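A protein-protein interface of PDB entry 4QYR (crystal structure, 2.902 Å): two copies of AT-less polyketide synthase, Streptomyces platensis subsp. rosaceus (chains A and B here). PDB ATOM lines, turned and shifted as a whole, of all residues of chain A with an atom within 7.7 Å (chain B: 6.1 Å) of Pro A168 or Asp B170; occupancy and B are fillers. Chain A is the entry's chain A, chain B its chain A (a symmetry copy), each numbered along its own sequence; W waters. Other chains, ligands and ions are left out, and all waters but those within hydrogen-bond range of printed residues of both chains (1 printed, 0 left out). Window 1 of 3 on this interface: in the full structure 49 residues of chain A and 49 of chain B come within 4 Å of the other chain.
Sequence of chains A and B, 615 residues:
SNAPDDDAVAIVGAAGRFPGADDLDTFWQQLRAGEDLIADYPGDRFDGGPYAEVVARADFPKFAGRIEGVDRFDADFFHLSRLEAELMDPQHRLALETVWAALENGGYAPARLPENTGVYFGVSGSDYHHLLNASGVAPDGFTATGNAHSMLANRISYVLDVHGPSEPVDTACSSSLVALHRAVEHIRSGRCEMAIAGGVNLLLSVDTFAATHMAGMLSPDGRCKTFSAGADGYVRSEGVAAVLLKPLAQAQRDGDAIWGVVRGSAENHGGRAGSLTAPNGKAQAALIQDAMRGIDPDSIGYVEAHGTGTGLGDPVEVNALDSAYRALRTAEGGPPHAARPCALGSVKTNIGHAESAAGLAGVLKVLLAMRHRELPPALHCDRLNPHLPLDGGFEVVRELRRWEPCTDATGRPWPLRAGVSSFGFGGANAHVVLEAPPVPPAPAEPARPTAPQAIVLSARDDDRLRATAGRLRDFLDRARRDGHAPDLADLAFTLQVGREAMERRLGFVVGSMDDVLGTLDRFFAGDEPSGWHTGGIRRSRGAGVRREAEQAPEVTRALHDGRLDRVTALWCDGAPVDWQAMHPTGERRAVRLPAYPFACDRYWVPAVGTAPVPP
Of the 13 printed residues of chain B, 4 touch a printed residue of chain A.
Printed residues of chain B that touch a printed residue of chain A: His B149, Pro B168, Asp B170 and Ala B172.
Hydrophobic or aromatic side chains of chain B that line the printed part of chain A: His B149 and Pro B168.
Of the 24 printed residues of chain A, 4 touch a printed residue of chain B.
Hydrophobic or aromatic side chains of chain A that line the printed part of chain B: His A149 and Pro A168.
Among the printed residues, no Asp or Glu carboxylate lies within 4 Å of a Lys or Arg side-chain nitrogen of the other chain.
Water W1 bridges ND2 of Asn A154 (2.6 Å) and O of Thr B171 (3.0 Å).
Asp B170 touches His A149.
Ala B172 touches Ser A150 (N to CB, 3.8 Å).
Pro A168 touches Asp B170 (CG to O, 3.1 Å).
Asp A170 touches His B149 (OD2 to CB, 3.6 Å).
Asp A170 touches Pro B168.
His A149 touches Asp B170, and with the chains exchanged Asp A170 touches His B149.
Pro A168 touches Asp B170, and with the chains exchanged Asp A170 touches Pro B168.
Positions printed for both chains: 121, 122, 123, 124, 149, 168, 169, 170, 171 and 175.
The backbone carbonyl oxygen (O) of Ser A124 lies within hydrogen-bond range of a ring nitrogen (NE2) of His A149 (3.3 Å).
The side-chain hydroxyl (OG) of Ser A124 sits at hydrogen-bond distance from the side-chain carboxylate (OD1) of Asp A170 (3.1 Å).
The side-chain amide nitrogen (ND2) of Asn A154 lies close to the backbone carbonyl oxygen (O) of Ser A150 (3.3 Å).
The backbone carbonyl oxygen of Ser B124 is in hydrogen-bond range of a ring nitrogen (NE2) of His B149 (3.3 Å).
The side-chain hydroxyl of Ser B124 lies within hydrogen-bond range of the backbone carbonyl oxygen of Ala B172, 3.5 Å away.
The backbone carbonyl oxygen (O) of Ala B172 is in hydrogen-bond range of the side-chain hydroxyl (OG) of Ser B175, at 2.9 Å.
Printed residues of chain B within 4 Å of His A149: Asp B170.
Of the printed residues of chain B, Ser A150 touches Asp B170 and Ala B172.
Of chain B, only Asp B170 (3.1 Å) comes within 4 Å of Pro A168.
Gly B125 touches none of the printed residues of chain A.
Of chain A, only His A149, Ser A150 and Pro A168 come within 4 Å of Asp B170.
The nearest residue of chain A that does not touch Asp B170 is Ala A148 (4.8 Å).
The nearest printed residue of chain B that does not touch Asp A170 is Val B169 (6.9 Å).
The side-chain hydroxyl of Ser A150 sits at hydrogen-bond distance from the side-chain carboxylate of Asp B170.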
ATOM      1  N   VAL A 119     -24.063  18.467   9.475  1.00  0.00           N
ATOM      2  CA  VAL A 119     -22.631  18.410   9.277  1.00  0.00           C
ATOM      3  C   VAL A 119     -22.035  17.421  10.257  1.00  0.00           C
ATOM      4  O   VAL A 119     -22.120  17.621  11.464  1.00  0.00           O
ATOM      5  CB  VAL A 119     -21.980  19.772   9.488  1.00  0.00           C
ATOM      6  CG1 VAL A 119     -20.465  19.626   9.467  1.00  0.00           C
ATOM      7  CG2 VAL A 119     -22.490  20.784   8.445  1.00  0.00           C
ATOM      8  N   TYR A 120     -21.443  16.352   9.729  1.00  0.00           N
ATOM      9  CA  TYR A 120     -20.910  15.253  10.541  1.00  0.00           C
ATOM     10  C   TYR A 120     -19.494  14.972  10.105  1.00  0.00           C
ATOM     11  O   TYR A 120     -19.272  14.472   9.012  1.00  0.00           O
ATOM     12  CB  TYR A 120     -21.763  14.004  10.392  1.00  0.00           C
ATOM     13  CG  TYR A 120     -23.238  14.275  10.494  1.00  0.00           C
ATOM     14  CD1 TYR A 120     -23.936  14.018  11.663  1.00  0.00           C
ATOM     15  CD2 TYR A 120     -23.939  14.785   9.411  1.00  0.00           C
ATOM     16  CE1 TYR A 120     -25.301  14.255  11.745  1.00  0.00           C
ATOM     17  CE2 TYR A 120     -25.290  15.025   9.477  1.00  0.00           C
ATOM     18  CZ  TYR A 120     -25.974  14.763  10.638  1.00  0.00           C
ATOM     19  OH  TYR A 120     -27.330  15.032  10.672  1.00  0.00           O
ATOM     20  N   PHE A 121     -18.527  15.307  10.938  1.00  0.00           N
ATOM     21  CA  PHE A 121     -17.151  15.279  10.476  1.00  0.00           C
ATOM     22  C   PHE A 121     -16.283  14.463  11.441  1.00  0.00           C
ATOM     23  O   PHE A 121     -16.292  14.693  12.651  1.00  0.00           O
ATOM     24  CB  PHE A 121     -16.635  16.699  10.345  1.00  0.00           C
ATOM     25  CG  PHE A 121     -15.641  16.880   9.262  1.00  0.00           C
ATOM     26  CD1 PHE A 121     -16.017  17.463   8.057  1.00  0.00           C
ATOM     27  CD2 PHE A 121     -14.325  16.484   9.431  1.00  0.00           C
ATOM     28  CE1 PHE A 121     -15.090  17.633   7.028  1.00  0.00           C
ATOM     29  CE2 PHE A 121     -13.392  16.656   8.404  1.00  0.00           C
ATOM     30  CZ  PHE A 121     -13.773  17.230   7.207  1.00  0.00           C
ATOM     31  N   GLY A 122     -15.545  13.493  10.913  1.00  0.00           N
ATOM     32  CA  GLY A 122     -14.784  12.604  11.772  1.00  0.00           C
ATOM     33  C   GLY A 122     -13.416  13.179  12.023  1.00  0.00           C
ATOM     34  O   GLY A 122     -12.804  13.738  11.110  1.00  0.00           O
ATOM     35  N   VAL A 123     -12.936  13.038  13.256  1.00  0.00           N
ATOM     36  CA  VAL A 123     -11.658  13.606  13.680  1.00  0.00           C
ATOM     37  C   VAL A 123     -11.267  12.950  14.995  1.00  0.00           C
ATOM     38  O   VAL A 123     -12.135  12.704  15.830  1.00  0.00           O
ATOM     39  CB  VAL A 123     -11.768  15.134  13.840  1.00  0.00           C
ATOM     40  CG1 VAL A 123     -12.942  15.475  14.733  1.00  0.00           C
ATOM     41  CG2 VAL A 123     -10.500  15.712  14.416  1.00  0.00           C
ATOM     42  N   SER A 124      -9.986  12.651  15.195  1.00  0.00           N
ATOM     43  CA  SER A 124      -9.579  11.941  16.414  1.00  0.00           C
ATOM     44  C   SER A 124      -8.515  12.625  17.264  1.00  0.00           C
ATOM     45  O   SER A 124      -8.624  12.648  18.483  1.00  0.00           O
ATOM     46  CB  SER A 124      -9.088  10.539  16.064  1.00  0.00           C
ATOM     47  OG  SER A 124     -10.161   9.759  15.561  1.00  0.00           O
ATOM     48  N   ASN A 147      -9.022  24.380  18.832  1.00  0.00           N
ATOM     49  CA  ASN A 147      -8.624  23.014  19.061  1.00  0.00           C
ATOM     50  C   ASN A 147      -9.670  22.090  19.622  1.00  0.00           C
ATOM     51  O   ASN A 147      -9.427  20.900  19.731  1.00  0.00           O
ATOM     52  CB  ASN A 147      -7.412  23.015  19.956  1.00  0.00           C
ATOM     53  CG  ASN A 147      -6.193  23.449  19.216  1.00  0.00           C
ATOM     54  OD1 ASN A 147      -5.602  22.654  18.476  1.00  0.00           O
ATOM     55  ND2 ASN A 147      -5.830  24.730  19.352  1.00  0.00           N
ATOM     56  N   ALA A 148     -10.834  22.615  19.960  1.00  0.00           N
ATOM     57  CA  ALA A 148     -11.929  21.762  20.383  1.00  0.00           C
ATOM     58  C   ALA A 148     -12.519  21.032  19.170  1.00  0.00           C
ATOM     59  O   ALA A 148     -12.744  21.642  18.124  1.00  0.00           O
ATOM     60  CB  ALA A 148     -12.976  22.587  21.080  1.00  0.00           C
ATOM     61  N   HIS A 149     -12.770  19.732  19.292  1.00  0.00           N
ATOM     62  CA  HIS A 149     -13.283  18.977  18.143  1.00  0.00           C
ATOM     63  C   HIS A 149     -14.652  19.477  17.692  1.00  0.00           C
ATOM     64  O   HIS A 149     -14.968  19.476  16.500  1.00  0.00           O
ATOM     65  CB  HIS A 149     -13.371  17.492  18.461  1.00  0.00           C
ATOM     66  CG  HIS A 149     -12.043  16.809  18.533  1.00  0.00           C
ATOM     67  ND1 HIS A 149     -10.892  17.369  18.028  1.00  0.00           N
ATOM     68  CD2 HIS A 149     -11.683  15.612  19.054  1.00  0.00           C
ATOM     69  CE1 HIS A 149      -9.878  16.548  18.235  1.00  0.00           C
ATOM     70  NE2 HIS A 149     -10.332  15.475  18.856  1.00  0.00           N
ATOM     71  N   SER A 150     -15.466  19.883  18.655  1.00  0.00           N
ATOM     72  CA  SER A 150     -16.753  20.486  18.357  1.00  0.00           C
ATOM     73  C   SER A 150     -16.625  21.637  17.382  1.00  0.00           C
ATOM     74  O   SER A 150     -17.474  21.828  16.514  1.00  0.00           O
ATOM     75  CB  SER A 150     -17.407  20.984  19.635  1.00  0.00           C
ATOM     76  OG  SER A 150     -16.411  21.464  20.522  1.00  0.00           O
ATOM     77  N   MET A 151     -15.553  22.403  17.511  1.00  0.00           N
ATOM     78  CA  MET A 151     -15.403  23.574  16.664  1.00  0.00           C
ATOM     79  C   MET A 151     -15.177  23.204  15.220  1.00  0.00           C
ATOM     80  O   MET A 151     -15.655  23.890  14.312  1.00  0.00           O
ATOM     81  CB  MET A 151     -14.275  24.467  17.167  1.00  0.00           C
ATOM     82  CG  MET A 151     -14.751  25.424  18.254  1.00  0.00           C
ATOM     83  SD  MET A 151     -16.335  26.429  17.683  1.00  0.00           S
ATOM     84  CE  MET A 151     -16.819  27.136  19.408  1.00  0.00           C
ATOM     85  N   LEU A 152     -14.469  22.109  15.004  1.00  0.00           N
ATOM     86  CA  LEU A 152     -14.274  21.625  13.660  1.00  0.00           C
ATOM     87  C   LEU A 152     -15.612  21.580  12.924  1.00  0.00           C
ATOM     88  O   LEU A 152     -15.732  22.096  11.821  1.00  0.00           O
ATOM     89  CB  LEU A 152     -13.625  20.253  13.679  1.00  0.00           C
ATOM     90  CG  LEU A 152     -13.067  19.737  12.357  1.00  0.00           C
ATOM     91  CD1 LEU A 152     -12.046  18.670  12.664  1.00  0.00           C
ATOM     92  CD2 LEU A 152     -14.143  19.163  11.513  1.00  0.00           C
ATOM     93  N   ALA A 153     -16.620  20.984  13.549  1.00  0.00           N
ATOM     94  CA  ALA A 153     -17.925  20.861  12.914  1.00  0.00           C
ATOM     95  C   ALA A 153     -18.674  22.183  12.964  1.00  0.00           C
ATOM     96  O   ALA A 153     -19.164  22.656  11.943  1.00  0.00           O
ATOM     97  CB  ALA A 153     -18.747  19.753  13.579  1.00  0.00           C
ATOM     98  N   ASN A 154     -18.756  22.786  14.144  1.00  0.00           N
ATOM     99  CA  ASN A 154     -19.596  23.965  14.311  1.00  0.00           C
ATOM    100  C   ASN A 154     -19.121  25.150  13.463  1.00  0.00           C
ATOM    101  O   ASN A 154     -19.927  25.893  12.903  1.00  0.00           O
ATOM    102  CB  ASN A 154     -19.668  24.372  15.790  1.00  0.00           C
ATOM    103  CG  ASN A 154     -20.253  23.274  16.686  1.00  0.00           C
ATOM    104  OD1 ASN A 154     -20.977  22.388  16.234  1.00  0.00           O
ATOM    105  ND2 ASN A 154     -19.950  23.351  17.970  1.00  0.00           N
ATOM    106  N   PRO A 165     -28.061  19.256  12.607  1.00  0.00           N
ATOM    107  CA  PRO A 165     -27.091  18.839  13.624  1.00  0.00           C
ATOM    108  C   PRO A 165     -25.649  19.012  13.141  1.00  0.00           C
ATOM    109  O   PRO A 165     -25.350  18.637  12.001  1.00  0.00           O
ATOM    110  CB  PRO A 165     -27.412  17.361  13.815  1.00  0.00           C
ATOM    111  CG  PRO A 165     -28.848  17.265  13.472  1.00  0.00           C
ATOM    112  CD  PRO A 165     -29.085  18.235  12.361  1.00  0.00           C
ATOM    113  N   SER A 166     -24.787  19.562  13.998  1.00  0.00           N
ATOM    114  CA  SER A 166     -23.365  19.766  13.712  1.00  0.00           C
ATOM    115  C   SER A 166     -22.505  18.982  14.699  1.00  0.00           C
ATOM    116  O   SER A 166     -22.394  19.345  15.856  1.00  0.00           O
ATOM    117  CB  SER A 166     -23.015  21.251  13.793  1.00  0.00           C
ATOM    118  OG  SER A 166     -21.690  21.522  13.336  1.00  0.00           O
ATOM    119  N   GLU A 167     -21.886  17.905  14.244  1.00  0.00           N
ATOM    120  CA  GLU A 167     -21.163  17.017  15.146  1.00  0.00           C
ATOM    121  C   GLU A 167     -19.800  16.587  14.619  1.00  0.00           C
ATOM    122  O   GLU A 167     -19.656  16.195  13.456  1.00  0.00           O
ATOM    123  CB  GLU A 167     -22.001  15.779  15.426  1.00  0.00           C
ATOM    124  CG  GLU A 167     -23.182  16.074  16.330  1.00  0.00           C
ATOM    125  CD  GLU A 167     -24.402  15.215  16.022  1.00  0.00           C
ATOM    126  OE1 GLU A 167     -24.392  14.499  14.978  1.00  0.00           O
ATOM    127  OE2 GLU A 167     -25.362  15.252  16.839  1.00  0.00           O
ATOM    128  N   PRO A 168     -18.788  16.668  15.479  1.00  0.00           N
ATOM    129  CA  PRO A 168     -17.606  15.839  15.271  1.00  0.00           C
ATOM    130  C   PRO A 168     -17.944  14.382  15.559  1.00  0.00           C
ATOM    131  O   PRO A 168     -18.844  14.080  16.351  1.00  0.00           O
ATOM    132  CB  PRO A 168     -16.605  16.385  16.274  1.00  0.00           C
ATOM    133  CG  PRO A 168     -17.422  17.004  17.317  1.00  0.00           C
ATOM    134  CD  PRO A 168     -18.704  17.463  16.703  1.00  0.00           C
ATOM    135  N   VAL A 169     -17.249  13.484  14.887  1.00  0.00           N
ATOM    136  CA  VAL A 169     -17.374  12.070  15.183  1.00  0.00           C
ATOM    137  C   VAL A 169     -16.004  11.493  15.549  1.00  0.00           C
ATOM    138  O   VAL A 169     -15.027  11.667  14.800  1.00  0.00           O
ATOM    139  CB  VAL A 169     -17.947  11.305  14.005  1.00  0.00           C
ATOM    140  CG1 VAL A 169     -17.863   9.818  14.282  1.00  0.00           C
ATOM    141  CG2 VAL A 169     -19.382  11.735  13.748  1.00  0.00           C
ATOM    142  N   ASP A 170     -15.926  10.837  16.709  1.00  0.00           N
ATOM    143  CA  ASP A 170     -14.672  10.219  17.149  1.00  0.00           C
ATOM    144  C   ASP A 170     -14.921   8.767  17.505  1.00  0.00           C
ATOM    145  O   ASP A 170     -15.237   8.459  18.646  1.00  0.00           O
ATOM    146  CB  ASP A 170     -14.058  10.955  18.353  1.00  0.00           C
ATOM    147  CG  ASP A 170     -12.624  10.487  18.676  1.00  0.00           C
ATOM    148  OD1 ASP A 170     -12.117   9.567  17.995  1.00  0.00           O
ATOM    149  OD2 ASP A 170     -12.011  11.024  19.632  1.00  0.00           O
ATOM    150  N   THR A 171     -14.789   7.883  16.522  1.00  0.00           N
ATOM    151  CA  THR A 171     -14.863   6.455  16.786  1.00  0.00           C
ATOM    152  C   THR A 171     -13.518   5.826  16.428  1.00  0.00           C
ATOM    153  O   THR A 171     -13.445   4.640  16.053  1.00  0.00           O
ATOM    154  CB  THR A 171     -16.002   5.789  16.001  1.00  0.00           C
ATOM    155  OG1 THR A 171     -15.725   5.892  14.601  1.00  0.00           O
ATOM    156  CG2 THR A 171     -17.329   6.458  16.312  1.00  0.00           C
ATOM    157  N   SER A 175     -13.991   6.774  12.148  1.00  0.00           N
ATOM    158  CA  SER A 175     -14.775   7.970  12.373  1.00  0.00           C
ATOM    159  C   SER A 175     -15.506   8.443  11.123  1.00  0.00           C
ATOM    160  O   SER A 175     -16.743   8.578  11.135  1.00  0.00           O
ATOM    161  CB  SER A 175     -13.891   9.066  12.930  1.00  0.00           C
ATOM    162  OG  SER A 175     -13.497   8.721  14.255  1.00  0.00           O
ATOM    163  N   ALA A 179     -19.484   8.846  10.270  1.00  0.00           N
ATOM    164  CA  ALA A 179     -20.008  10.121   9.819  1.00  0.00           C
ATOM    165  C   ALA A 179     -20.986   9.911   8.688  1.00  0.00           C
ATOM    166  O   ALA A 179     -22.153  10.287   8.776  1.00  0.00           O
ATOM    167  CB  ALA A 179     -18.883  11.024   9.361  1.00  0.00           C
ATOM    168  N   GLY A 198     -17.688  14.103   6.486  1.00  0.00           N
ATOM    169  CA  GLY A 198     -16.276  14.249   6.189  1.00  0.00           C
ATOM    170  C   GLY A 198     -15.401  13.597   7.241  1.00  0.00           C
ATOM    171  O   GLY A 198     -15.881  13.095   8.281  1.00  0.00           O
ATOM    172  N   PHE B 121     -21.895   9.051  25.140  1.00  0.00           N
ATOM    173  CA  PHE B 121     -21.386   9.712  26.328  1.00  0.00           C
ATOM    174  C   PHE B 121     -20.724  11.042  25.953  1.00  0.00           C
ATOM    175  O   PHE B 121     -19.868  11.097  25.069  1.00  0.00           O
ATOM    176  CB  PHE B 121     -20.407   8.794  27.036  1.00  0.00           C
ATOM    177  CG  PHE B 121     -20.390   8.954  28.507  1.00  0.00           C
ATOM    178  CD1 PHE B 121     -21.035   8.027  29.319  1.00  0.00           C
ATOM    179  CD2 PHE B 121     -19.728  10.015  29.101  1.00  0.00           C
ATOM    180  CE1 PHE B 121     -21.031   8.170  30.707  1.00  0.00           C
ATOM    181  CE2 PHE B 121     -19.717  10.161  30.491  1.00  0.00           C
ATOM    182  CZ  PHE B 121     -20.365   9.240  31.292  1.00  0.00           C
ATOM    183  N   GLY B 122     -21.132  12.124  26.607  1.00  0.00           N
ATOM    184  CA  GLY B 122     -20.634  13.435  26.233  1.00  0.00           C
ATOM    185  C   GLY B 122     -19.374  13.744  26.996  1.00  0.00           C
ATOM    186  O   GLY B 122     -19.276  13.424  28.182  1.00  0.00           O
ATOM    187  N   VAL B 123     -18.416  14.369  26.316  1.00  0.00           N
ATOM    188  CA  VAL B 123     -17.105  14.671  26.889  1.00  0.00           C
ATOM    189  C   VAL B 123     -16.423  15.688  25.988  1.00  0.00           C
ATOM    190  O   VAL B 123     -16.552  15.599  24.769  1.00  0.00           O
ATOM    191  CB  VAL B 123     -16.257  13.391  27.014  1.00  0.00           C
ATOM    192  CG1 VAL B 123     -16.217  12.669  25.684  1.00  0.00           C
ATOM    193  CG2 VAL B 123     -14.855  13.712  27.466  1.00  0.00           C
ATOM    194  N   SER B 124     -15.710  16.657  26.557  1.00  0.00           N
ATOM    195  CA  SER B 124     -15.106  17.707  25.727  1.00  0.00           C
ATOM    196  C   SER B 124     -13.599  17.888  25.867  1.00  0.00           C
ATOM    197  O   SER B 124     -12.906  18.061  24.873  1.00  0.00           O
ATOM    198  CB  SER B 124     -15.780  19.049  26.006  1.00  0.00           C
ATOM    199  OG  SER B 124     -17.131  19.013  25.575  1.00  0.00           O
ATOM    200  N   GLY B 125     -13.074  17.860  27.081  1.00  0.00           N
ATOM    201  CA  GLY B 125     -11.681  18.209  27.251  1.00  0.00           C
ATOM    202  C   GLY B 125     -10.727  17.053  27.371  1.00  0.00           C
ATOM    203  O   GLY B 125     -11.092  15.989  27.847  1.00  0.00           O
ATOM    204  N   HIS B 149     -11.063  10.203  23.177  1.00  0.00           N
ATOM    205  CA  HIS B 149     -12.468  10.313  23.588  1.00  0.00           C
ATOM    206  C   HIS B 149     -13.278   9.081  23.199  1.00  0.00           C
ATOM    207  O   HIS B 149     -14.192   8.668  23.917  1.00  0.00           O
ATOM    208  CB  HIS B 149     -13.116  11.550  22.985  1.00  0.00           C
ATOM    209  CG  HIS B 149     -12.660  12.834  23.601  1.00  0.00           C
ATOM    210  ND1 HIS B 149     -11.995  12.884  24.805  1.00  0.00           N
ATOM    211  CD2 HIS B 149     -12.767  14.115  23.177  1.00  0.00           C
ATOM    212  CE1 HIS B 149     -11.713  14.141  25.097  1.00  0.00           C
ATOM    213  NE2 HIS B 149     -12.171  14.907  24.125  1.00  0.00           N
ATOM    214  N   PRO B 168     -18.549   8.727  21.788  1.00  0.00           N
ATOM    215  CA  PRO B 168     -18.425   9.994  22.499  1.00  0.00           C
ATOM    216  C   PRO B 168     -19.224  11.070  21.773  1.00  0.00           C
ATOM    217  O   PRO B 168     -19.428  11.000  20.555  1.00  0.00           O
ATOM    218  CB  PRO B 168     -16.935  10.287  22.455  1.00  0.00           C
ATOM    219  CG  PRO B 168     -16.447   9.557  21.286  1.00  0.00           C
ATOM    220  CD  PRO B 168     -17.328   8.370  21.066  1.00  0.00           C
ATOM    221  N   VAL B 169     -19.706  12.039  22.526  1.00  0.00           N
ATOM    222  CA  VAL B 169     -20.353  13.193  21.933  1.00  0.00           C
ATOM    223  C   VAL B 169     -19.634  14.472  22.371  1.00  0.00           C
ATOM    224  O   VAL B 169     -19.427  14.696  23.577  1.00  0.00           O
ATOM    225  CB  VAL B 169     -21.815  13.274  22.328  1.00  0.00           C
ATOM    226  CG1 VAL B 169     -22.390  14.596  21.861  1.00  0.00           C
ATOM    227  CG2 VAL B 169     -22.584  12.103  21.736  1.00  0.00           C
ATOM    228  N   ASP B 170     -19.230  15.291  21.398  1.00  0.00           N
ATOM    229  CA  ASP B 170     -18.556  16.558  21.700  1.00  0.00           C
ATOM    230  C   ASP B 170     -19.258  17.689  20.978  1.00  0.00           C
ATOM    231  O   ASP B 170     -18.911  18.008  19.849  1.00  0.00           O
ATOM    232  CB  ASP B 170     -17.069  16.528  21.306  1.00  0.00           C
ATOM    233  CG  ASP B 170     -16.281  17.743  21.838  1.00  0.00           C
ATOM    234  OD1 ASP B 170     -16.892  18.628  22.480  1.00  0.00           O
ATOM    235  OD2 ASP B 170     -15.052  17.825  21.592  1.00  0.00           O
ATOM    236  N   THR B 171     -20.253  18.283  21.629  1.00  0.00           N
ATOM    237  CA  THR B 171     -20.896  19.470  21.088  1.00  0.00           C
ATOM    238  C   THR B 171     -20.663  20.630  22.055  1.00  0.00           C
ATOM    239  O   THR B 171     -21.481  21.565  22.143  1.00  0.00           O
ATOM    240  CB  THR B 171     -22.397  19.249  20.856  1.00  0.00           C
ATOM    241  OG1 THR B 171     -23.035  19.023  22.116  1.00  0.00           O
ATOM    242  CG2 THR B 171     -22.628  18.056  19.945  1.00  0.00           C
ATOM    243  N   ALA B 172     -19.536  20.529  22.767  1.00  0.00           N
ATOM    244  CA  ALA B 172     -19.128  21.468  23.804  1.00  0.00           C
ATOM    245  C   ALA B 172     -20.103  21.443  24.977  1.00  0.00           C
ATOM    246  O   ALA B 172     -20.284  20.425  25.623  1.00  0.00           O
ATOM    247  CB  ALA B 172     -18.990  22.875  23.240  1.00  0.00           C
ATOM    248  N   SER B 175     -23.048  18.721  25.233  1.00  0.00           N
ATOM    249  CA  SER B 175     -22.733  17.367  24.828  1.00  0.00           C
ATOM    250  C   SER B 175     -23.672  16.332  25.435  1.00  0.00           C
ATOM    251  O   SER B 175     -24.317  15.565  24.697  1.00  0.00           O
ATOM    252  CB  SER B 175     -21.291  17.053  25.167  1.00  0.00           C
ATOM    253  OG  SER B 175     -20.434  17.818  24.323  1.00  0.00           O
ATOM    254  N   SER B 356     -19.674  19.798  29.488  1.00  0.00           N
ATOM    255  CA  SER B 356     -20.155  18.526  28.910  1.00  0.00           C
ATOM    256  C   SER B 356     -21.164  17.753  29.769  1.00  0.00           C
ATOM    257  O   SER B 356     -21.924  16.944  29.256  1.00  0.00           O
ATOM    258  CB  SER B 356     -18.990  17.595  28.625  1.00  0.00           C
ATOM    259  OG  SER B 356     -17.953  18.327  28.032  1.00  0.00           O
HETATM  260  O   HOH W   1     -21.225  23.887  20.204  1.00  0.00           O
